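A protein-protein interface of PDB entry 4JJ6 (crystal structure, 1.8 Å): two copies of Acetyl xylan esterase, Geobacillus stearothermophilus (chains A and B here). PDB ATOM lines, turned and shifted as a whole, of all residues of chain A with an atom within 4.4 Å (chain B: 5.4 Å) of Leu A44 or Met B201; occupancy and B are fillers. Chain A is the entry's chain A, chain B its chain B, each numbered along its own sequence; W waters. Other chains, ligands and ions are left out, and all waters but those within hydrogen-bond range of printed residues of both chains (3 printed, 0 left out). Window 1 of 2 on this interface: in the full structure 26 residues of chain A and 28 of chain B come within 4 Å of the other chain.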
ATOM      1  N   TYR A  40     -14.729  10.289  19.850  1.00  0.00           N
ATOM      2  CA  TYR A  40     -14.070  11.082  18.896  1.00  0.00           C
ATOM      3  C   TYR A  40     -13.582  10.190  17.734  1.00  0.00           C
ATOM      4  O   TYR A  40     -13.631  10.607  16.568  1.00  0.00           O
ATOM      5  CB  TYR A  40     -12.889  11.825  19.476  1.00  0.00           C
ATOM      6  CG  TYR A  40     -13.231  12.821  20.626  1.00  0.00           C
ATOM      7  CD1 TYR A  40     -14.520  13.254  20.843  1.00  0.00           C
ATOM      8  CD2 TYR A  40     -12.242  13.374  21.311  1.00  0.00           C
ATOM      9  CE1 TYR A  40     -14.827  14.195  21.882  1.00  0.00           C
ATOM     10  CE2 TYR A  40     -12.482  14.272  22.330  1.00  0.00           C
ATOM     11  CZ  TYR A  40     -13.779  14.704  22.585  1.00  0.00           C
ATOM     12  OH  TYR A  40     -13.940  15.617  23.596  1.00  0.00           O
ATOM     13  N   VAL A  41     -13.072   9.011  18.078  1.00  0.00           N
ATOM     14  CA  VAL A  41     -12.711   8.048  17.093  1.00  0.00           C
ATOM     15  C   VAL A  41     -13.863   7.718  16.177  1.00  0.00           C
ATOM     16  O   VAL A  41     -13.694   7.777  14.958  1.00  0.00           O
ATOM     17  CB  VAL A  41     -12.088   6.818  17.734  1.00  0.00           C
ATOM     18  CG1 VAL A  41     -11.980   5.713  16.684  1.00  0.00           C
ATOM     19  CG2 VAL A  41     -10.736   7.171  18.339  1.00  0.00           C
ATOM     20  N   VAL A  42     -15.012   7.413  16.730  1.00  0.00           N
ATOM     21  CA  VAL A  42     -16.183   7.003  15.951  1.00  0.00           C
ATOM     22  C   VAL A  42     -16.650   8.191  15.089  1.00  0.00           C
ATOM     23  O   VAL A  42     -16.943   8.031  13.867  1.00  0.00           O
ATOM     24  CB  VAL A  42     -17.280   6.453  16.839  1.00  0.00           C
ATOM     25  CG1 VAL A  42     -18.514   6.071  16.028  1.00  0.00           C
ATOM     26  CG2 VAL A  42     -16.780   5.224  17.605  1.00  0.00           C
ATOM     27  N   GLY A  43     -16.629   9.403  15.653  1.00  0.00           N
ATOM     28  CA  GLY A  43     -16.940  10.560  14.856  1.00  0.00           C
ATOM     29  C   GLY A  43     -16.049  10.872  13.696  1.00  0.00           C
ATOM     30  O   GLY A  43     -16.543  11.262  12.630  1.00  0.00           O
ATOM     31  N   LEU A  44     -14.742  10.749  13.877  1.00  0.00           N
ATOM     32  CA  LEU A  44     -13.841  11.021  12.799  1.00  0.00           C
ATOM     33  C   LEU A  44     -13.913   9.940  11.731  1.00  0.00           C
ATOM     34  O   LEU A  44     -13.792  10.239  10.556  1.00  0.00           O
ATOM     35  CB  LEU A  44     -12.396  11.191  13.310  1.00  0.00           C
ATOM     36  CG  LEU A  44     -12.157  12.551  13.950  1.00  0.00           C
ATOM     37  CD1 LEU A  44     -10.913  12.545  14.809  1.00  0.00           C
ATOM     38  CD2 LEU A  44     -12.111  13.629  12.885  1.00  0.00           C
ATOM     39  N   LEU A  45     -14.242   8.722  12.127  1.00  0.00           N
ATOM     40  CA  LEU A  45     -14.326   7.647  11.172  1.00  0.00           C
ATOM     41  C   LEU A  45     -15.554   7.838  10.337  1.00  0.00           C
ATOM     42  O   LEU A  45     -15.525   7.605   9.115  1.00  0.00           O
ATOM     43  CB  LEU A  45     -14.398   6.305  11.899  1.00  0.00           C
ATOM     44  CG  LEU A  45     -13.031   5.799  12.374  1.00  0.00           C
ATOM     45  CD1 LEU A  45     -13.220   4.549  13.190  1.00  0.00           C
ATOM     46  CD2 LEU A  45     -12.064   5.523  11.224  1.00  0.00           C
ATOM     47  N   GLN A  46     -16.606   8.312  10.994  1.00  0.00           N
ATOM     48  CA  GLN A  46     -17.839   8.592  10.317  1.00  0.00           C
ATOM     49  C   GLN A  46     -17.706   9.800   9.367  1.00  0.00           C
ATOM     50  O   GLN A  46     -18.335   9.795   8.284  1.00  0.00           O
ATOM     51  CB  GLN A  46     -18.967   8.666  11.311  1.00  0.00           C
ATOM     52  CG  GLN A  46     -20.330   8.715  10.689  1.00  0.00           C
ATOM     53  CD  GLN A  46     -21.402   8.253  11.673  1.00  0.00           C
ATOM     54  OE1 GLN A  46     -21.435   8.667  12.846  1.00  0.00           O
ATOM     55  NE2 GLN A  46     -22.232   7.331  11.220  1.00  0.00           N
ATOM     56  N   ALA A  47     -16.969  10.826   9.790  1.00  0.00           N
ATOM     57  CA  ALA A  47     -16.763  12.022   8.995  1.00  0.00           C
ATOM     58  C   ALA A  47     -15.946  11.755   7.761  1.00  0.00           C
ATOM     59  O   ALA A  47     -16.149  12.435   6.735  1.00  0.00           O
ATOM     60  CB  ALA A  47     -16.056  13.120   9.757  1.00  0.00           C
ATOM     61  N   VAL A  48     -14.946  10.869   7.890  1.00  0.00           N
ATOM     62  CA  VAL A  48     -13.992  10.673   6.820  1.00  0.00           C
ATOM     63  C   VAL A  48     -14.210   9.350   6.023  1.00  0.00           C
ATOM     64  O   VAL A  48     -13.899   9.299   4.862  1.00  0.00           O
ATOM     65  CB  VAL A  48     -12.560  10.809   7.382  1.00  0.00           C
ATOM     66  CG1 VAL A  48     -11.560  10.688   6.245  1.00  0.00           C
ATOM     67  CG2 VAL A  48     -12.394  12.137   8.114  1.00  0.00           C
ATOM     68  N   MET A 201      -8.372  14.126  22.429  1.00  0.00           N
ATOM     69  CA  MET A 201      -7.942  14.243  21.021  1.00  0.00           C
ATOM     70  C   MET A 201      -6.547  13.667  20.798  1.00  0.00           C
ATOM     71  O   MET A 201      -6.305  13.031  19.748  1.00  0.00           O
ATOM     72  CB  MET A 201      -7.924  15.711  20.556  1.00  0.00           C
ATOM     73  CG  MET A 201      -9.307  16.222  20.255  1.00  0.00           C
ATOM     74  SD  MET A 201     -10.213  15.401  18.978  1.00  0.00           S
ATOM     75  CE  MET A 201     -11.668  16.416  19.151  1.00  0.00           C
ATOM     76  N   LEU A 208      -6.080   6.509  15.842  1.00  0.00           N
ATOM     77  CA  LEU A 208      -6.385   6.583  14.438  1.00  0.00           C
ATOM     78  C   LEU A 208      -5.149   6.427  13.595  1.00  0.00           C
ATOM     79  O   LEU A 208      -5.221   5.779  12.531  1.00  0.00           O
ATOM     80  CB  LEU A 208      -7.077   7.951  14.217  1.00  0.00           C
ATOM     81  CG  LEU A 208      -8.576   7.935  14.614  1.00  0.00           C
ATOM     82  CD1 LEU A 208      -9.138   9.350  14.573  1.00  0.00           C
ATOM     83  CD2 LEU A 208      -9.478   7.023  13.804  1.00  0.00           C
ATOM     84  N   PHE A 213      -5.829   5.565   9.592  1.00  0.00           N
ATOM     85  CA  PHE A 213      -6.695   6.712   9.229  1.00  0.00           C
ATOM     86  C   PHE A 213      -5.952   7.772   8.483  1.00  0.00           C
ATOM     87  O   PHE A 213      -4.788   8.142   8.809  1.00  0.00           O
ATOM     88  CB  PHE A 213      -7.342   7.263  10.536  1.00  0.00           C
ATOM     89  CG  PHE A 213      -8.098   8.572  10.403  1.00  0.00           C
ATOM     90  CD1 PHE A 213      -9.437   8.573  10.241  1.00  0.00           C
ATOM     91  CD2 PHE A 213      -7.451   9.746  10.610  1.00  0.00           C
ATOM     92  CE1 PHE A 213     -10.123   9.757  10.231  1.00  0.00           C
ATOM     93  CE2 PHE A 213      -8.112  10.967  10.575  1.00  0.00           C
ATOM     94  CZ  PHE A 213      -9.461  10.937  10.336  1.00  0.00           C
ATOM     95  N   TRP A 215      -6.544  11.789   7.420  1.00  0.00           N
ATOM     96  CA  TRP A 215      -7.303  13.036   7.645  1.00  0.00           C
ATOM     97  C   TRP A 215      -7.977  13.504   6.348  1.00  0.00           C
ATOM     98  O   TRP A 215      -9.158  13.813   6.299  1.00  0.00           O
ATOM     99  CB  TRP A 215      -6.359  14.081   8.140  1.00  0.00           C
ATOM    100  CG  TRP A 215      -6.919  15.437   8.395  1.00  0.00           C
ATOM    101  CD1 TRP A 215      -6.652  16.561   7.683  1.00  0.00           C
ATOM    102  CD2 TRP A 215      -7.881  15.823   9.424  1.00  0.00           C
ATOM    103  NE1 TRP A 215      -7.333  17.654   8.225  1.00  0.00           N
ATOM    104  CE2 TRP A 215      -8.088  17.230   9.287  1.00  0.00           C
ATOM    105  CE3 TRP A 215      -8.468  15.148  10.515  1.00  0.00           C
ATOM    106  CZ2 TRP A 215      -8.861  17.974  10.199  1.00  0.00           C
ATOM    107  CZ3 TRP A 215      -9.246  15.862  11.387  1.00  0.00           C
ATOM    108  CH2 TRP A 215      -9.457  17.274  11.206  1.00  0.00           C
ATOM    109  N   TYR B  40     -13.953  20.866  19.799  1.00  0.00           N
ATOM    110  CA  TYR B  40     -13.112  19.893  19.017  1.00  0.00           C
ATOM    111  C   TYR B  40     -11.990  20.644  18.296  1.00  0.00           C
ATOM    112  O   TYR B  40     -10.838  20.184  18.282  1.00  0.00           O
ATOM    113  CB  TYR B  40     -13.962  19.124  18.039  1.00  0.00           C
ATOM    114  CG  TYR B  40     -15.075  18.283  18.616  1.00  0.00           C
ATOM    115  CD1 TYR B  40     -15.190  18.019  19.992  1.00  0.00           C
ATOM    116  CD2 TYR B  40     -15.984  17.694  17.805  1.00  0.00           C
ATOM    117  CE1 TYR B  40     -16.186  17.186  20.492  1.00  0.00           C
ATOM    118  CE2 TYR B  40     -16.976  16.907  18.278  1.00  0.00           C
ATOM    119  CZ  TYR B  40     -17.118  16.687  19.663  1.00  0.00           C
ATOM    120  OH  TYR B  40     -18.146  15.902  20.164  1.00  0.00           O
ATOM    121  N   LEU B  44      -8.094  19.846  18.977  1.00  0.00           N
ATOM    122  CA  LEU B  44      -7.146  19.455  17.932  1.00  0.00           C
ATOM    123  C   LEU B  44      -6.007  20.441  17.818  1.00  0.00           C
ATOM    124  O   LEU B  44      -4.856  20.023  17.659  1.00  0.00           O
ATOM    125  CB  LEU B  44      -7.894  19.240  16.627  1.00  0.00           C
ATOM    126  CG  LEU B  44      -8.578  17.894  16.617  1.00  0.00           C
ATOM    127  CD1 LEU B  44      -9.641  17.872  15.547  1.00  0.00           C
ATOM    128  CD2 LEU B  44      -7.567  16.763  16.477  1.00  0.00           C
ATOM    129  N   SER B 196     -24.937  14.810  16.050  1.00  0.00           N
ATOM    130  CA  SER B 196     -24.076  13.895  16.792  1.00  0.00           C
ATOM    131  C   SER B 196     -22.615  14.406  16.902  1.00  0.00           C
ATOM    132  O   SER B 196     -22.219  15.420  16.269  1.00  0.00           O
ATOM    133  CB  SER B 196     -24.066  12.539  15.950  1.00  0.00           C
ATOM    134  OG  SER B 196     -23.618  12.833  14.573  1.00  0.00           O
ATOM    135  N   VAL B 197     -21.827  13.692  17.688  1.00  0.00           N
ATOM    136  CA  VAL B 197     -20.357  13.945  17.713  1.00  0.00           C
ATOM    137  C   VAL B 197     -19.903  13.903  16.233  1.00  0.00           C
ATOM    138  O   VAL B 197     -19.064  14.715  15.810  1.00  0.00           O
ATOM    139  CB  VAL B 197     -19.686  12.867  18.511  1.00  0.00           C
ATOM    140  CG1 VAL B 197     -18.135  12.976  18.363  1.00  0.00           C
ATOM    141  CG2 VAL B 197     -20.111  12.948  20.015  1.00  0.00           C
ATOM    142  N   ALA B 198     -20.371  12.927  15.466  1.00  0.00           N
ATOM    143  CA  ALA B 198     -19.913  12.865  14.058  1.00  0.00           C
ATOM    144  C   ALA B 198     -20.129  14.156  13.290  1.00  0.00           C
ATOM    145  O   ALA B 198     -19.251  14.608  12.633  1.00  0.00           O
ATOM    146  CB  ALA B 198     -20.527  11.724  13.282  1.00  0.00           C
ATOM    147  N   GLY B 199     -21.325  14.716  13.362  1.00  0.00           N
ATOM    148  CA  GLY B 199     -21.604  16.025  12.755  1.00  0.00           C
ATOM    149  C   GLY B 199     -20.727  17.135  13.186  1.00  0.00           C
ATOM    150  O   GLY B 199     -20.336  17.959  12.386  1.00  0.00           O
ATOM    151  N   HIS B 200     -20.448  17.204  14.495  1.00  0.00           N
ATOM    152  CA  HIS B 200     -19.532  18.157  14.994  1.00  0.00           C
ATOM    153  C   HIS B 200     -18.143  17.924  14.528  1.00  0.00           C
ATOM    154  O   HIS B 200     -17.387  18.890  14.341  1.00  0.00           O
ATOM    155  CB  HIS B 200     -19.676  18.338  16.553  1.00  0.00           C
ATOM    156  CG  HIS B 200     -20.828  19.200  16.926  1.00  0.00           C
ATOM    157  ND1 HIS B 200     -22.087  18.715  17.215  1.00  0.00           N
ATOM    158  CD2 HIS B 200     -20.943  20.549  16.903  1.00  0.00           C
ATOM    159  CE1 HIS B 200     -22.918  19.735  17.372  1.00  0.00           C
ATOM    160  NE2 HIS B 200     -22.254  20.843  17.181  1.00  0.00           N
ATOM    161  N   MET B 201     -17.757  16.664  14.363  1.00  0.00           N
ATOM    162  CA  MET B 201     -16.430  16.413  13.783  1.00  0.00           C
ATOM    163  C   MET B 201     -16.370  16.823  12.299  1.00  0.00           C
ATOM    164  O   MET B 201     -15.345  17.314  11.836  1.00  0.00           O
ATOM    165  CB  MET B 201     -16.108  14.926  13.855  1.00  0.00           C
ATOM    166  CG  MET B 201     -15.622  14.521  15.165  1.00  0.00           C
ATOM    167  SD  MET B 201     -14.088  15.318  15.726  1.00  0.00           S
ATOM    168  CE  MET B 201     -14.049  14.321  17.213  1.00  0.00           C
ATOM    169  N   ILE B 202     -17.464  16.649  11.581  1.00  0.00           N
ATOM    170  CA  ILE B 202     -17.528  17.063  10.152  1.00  0.00           C
ATOM    171  C   ILE B 202     -17.277  18.580  10.085  1.00  0.00           C
ATOM    172  O   ILE B 202     -16.492  19.096   9.268  1.00  0.00           O
ATOM    173  CB  ILE B 202     -18.890  16.711   9.510  1.00  0.00           C
ATOM    174  CG1 ILE B 202     -18.987  15.187   9.308  1.00  0.00           C
ATOM    175  CG2 ILE B 202     -19.142  17.500   8.254  1.00  0.00           C
ATOM    176  CD1 ILE B 202     -20.359  14.672   8.949  1.00  0.00           C
ATOM    177  N   LEU B 203     -17.915  19.271  10.981  1.00  0.00           N
ATOM    178  CA  LEU B 203     -17.760  20.745  11.053  1.00  0.00           C
ATOM    179  C   LEU B 203     -16.403  21.174  11.492  1.00  0.00           C
ATOM    180  O   LEU B 203     -15.778  22.080  10.913  1.00  0.00           O
ATOM    181  CB  LEU B 203     -18.776  21.301  12.018  1.00  0.00           C
ATOM    182  CG  LEU B 203     -20.254  21.290  11.565  1.00  0.00           C
ATOM    183  CD1 LEU B 203     -21.172  21.609  12.692  1.00  0.00           C
ATOM    184  CD2 LEU B 203     -20.414  22.317  10.508  1.00  0.00           C
ATOM    185  N   ALA B 204     -15.938  20.565  12.564  1.00  0.00           N
ATOM    186  CA  ALA B 204     -14.568  20.866  13.051  1.00  0.00           C
ATOM    187  C   ALA B 204     -13.482  20.667  11.969  1.00  0.00           C
ATOM    188  O   ALA B 204     -12.590  21.505  11.771  1.00  0.00           O
ATOM    189  CB  ALA B 204     -14.271  20.047  14.287  1.00  0.00           C
ATOM    190  N   ARG B 205     -13.541  19.534  11.327  1.00  0.00           N
ATOM    191  CA  ARG B 205     -12.630  19.235  10.233  1.00  0.00           C
ATOM    192  C   ARG B 205     -12.716  20.207   9.083  1.00  0.00           C
ATOM    193  O   ARG B 205     -11.719  20.620   8.564  1.00  0.00           O
ATOM    194  CB  ARG B 205     -12.872  17.822   9.757  1.00  0.00           C
ATOM    195  CG  ARG B 205     -12.072  17.444   8.522  1.00  0.00           C
ATOM    196  CD  ARG B 205     -12.167  15.942   8.407  1.00  0.00           C
ATOM    197  NE  ARG B 205     -11.483  15.427   7.203  1.00  0.00           N
ATOM    198  CZ  ARG B 205     -12.120  15.176   6.075  1.00  0.00           C
ATOM    199  NH1 ARG B 205     -13.424  15.508   5.918  1.00  0.00           N
ATOM    200  NH2 ARG B 205     -11.433  14.610   5.049  1.00  0.00           N
ATOM    201  N   ALA B 206     -13.935  20.525   8.673  1.00  0.00           N
ATOM    202  CA  ALA B 206     -14.144  21.548   7.611  1.00  0.00           C
ATOM    203  C   ALA B 206     -13.479  22.909   7.993  1.00  0.00           C
ATOM    204  O   ALA B 206     -12.736  23.543   7.178  1.00  0.00           O
ATOM    205  CB  ALA B 206     -15.617  21.668   7.275  1.00  0.00           C
ATOM    206  N   TRP B 215      -2.901  17.527  10.069  1.00  0.00           N
ATOM    207  CA  TRP B 215      -3.115  16.424  10.999  1.00  0.00           C
ATOM    208  C   TRP B 215      -1.799  15.837  11.526  1.00  0.00           C
ATOM    209  O   TRP B 215      -1.626  15.638  12.744  1.00  0.00           O
ATOM    210  CB  TRP B 215      -3.980  15.430  10.327  1.00  0.00           C
ATOM    211  CG  TRP B 215      -4.206  14.117  11.025  1.00  0.00           C
ATOM    212  CD1 TRP B 215      -3.601  12.917  10.712  1.00  0.00           C
ATOM    213  CD2 TRP B 215      -5.121  13.842  12.114  1.00  0.00           C
ATOM    214  NE1 TRP B 215      -4.117  11.902  11.507  1.00  0.00           N
ATOM    215  CE2 TRP B 215      -5.058  12.437  12.363  1.00  0.00           C
ATOM    216  CE3 TRP B 215      -6.067  14.632  12.830  1.00  0.00           C
ATOM    217  CZ2 TRP B 215      -5.807  11.819  13.361  1.00  0.00           C
ATOM    218  CZ3 TRP B 215      -6.860  14.001  13.773  1.00  0.00           C
ATOM    219  CH2 TRP B 215      -6.734  12.611  14.044  1.00  0.00           C
HETATM  220  O   HOH W   1     -23.748  10.211  13.629  1.00  0.00           O
HETATM  221  O   HOH W   2     -16.649  15.260   6.460  1.00  0.00           O
HETATM  222  O   HOH W   3      -3.343   9.327  10.524  1.00  0.00           O
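Tyr A40 touches its own counterpart, Tyr B40. Tyr A40 touches Met B201, and with the chains exchanged Met A201 touches Tyr B40. Met B201 touches its own counterpart, Met A201. Trp B215 touches its own counterpart, Trp A215. 4 positions are printed for both chains.
O of Leu A208 sits at hydrogen-bond distance from N of Phe A213 (3.0 Å). The side-chain hydroxyl (OG) of Ser B196 sits close to the backbone NH (N) of Ala B198 (3.4 Å).
Among the printed residues, pairs that only touch across the chains: Tyr A40 with Tyr B40, Tyr A40 with Met B201, Gly A43 with Ala B198, Gly A43 with Met B201, Leu A44 with Met B201, Gln A46 with Ala B198, Ala A47 with Ile B202, Val A48 with Arg B205, Met A201 with Tyr B40, Met A201 with Leu B44, Met A201 with Met B201, Phe A213 with Trp B215 and Trp A215 with Trp B215.
O of Trp A215 sits at hydrogen-bond distance from NH2 of Arg B205 (2.7 Å).
Printed residues of chain B that touch a printed residue of chain A: Tyr B40, Leu B44, Ala B198, Met B201, Ile B202, Arg B205 and Trp B215. Hydrophobic or aromatic side chains of chain A within 4 Å of the printed part of chain B: Tyr A40, Leu A44, Ala A47, Val A48, Met A201, Phe A213 and Trp A215.
Leu A44 touches just one residue of chain B: Met B201. Printed residues of chain A within 4 Å of Met B201: Tyr A40, Gly A43, Leu A44 and Met A201. Of the printed residues of chain B, Met A201 touches Tyr B40 (3.7 Å), Leu B44 (3.8 Å) and Met B201 (3.7 Å). Printed residues of chain A within 4 Å of Tyr B40: Tyr A40 (3.6 Å) and Met A201 (3.7 Å).
Water W3 bridges the backbone carbonyl oxygen of Phe A213 (2.5 Å) and the indole nitrogen of Trp B215 (2.9 Å). Water W1 lies within hydrogen-bond range of OG of Ser B196 and OE1 of Gln A46. Water W2 bridges the backbone carbonyl oxygen (O) of Ala A47 (2.9 Å) and the guanidinium group (NH1) of Arg B205 (3.3 Å).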
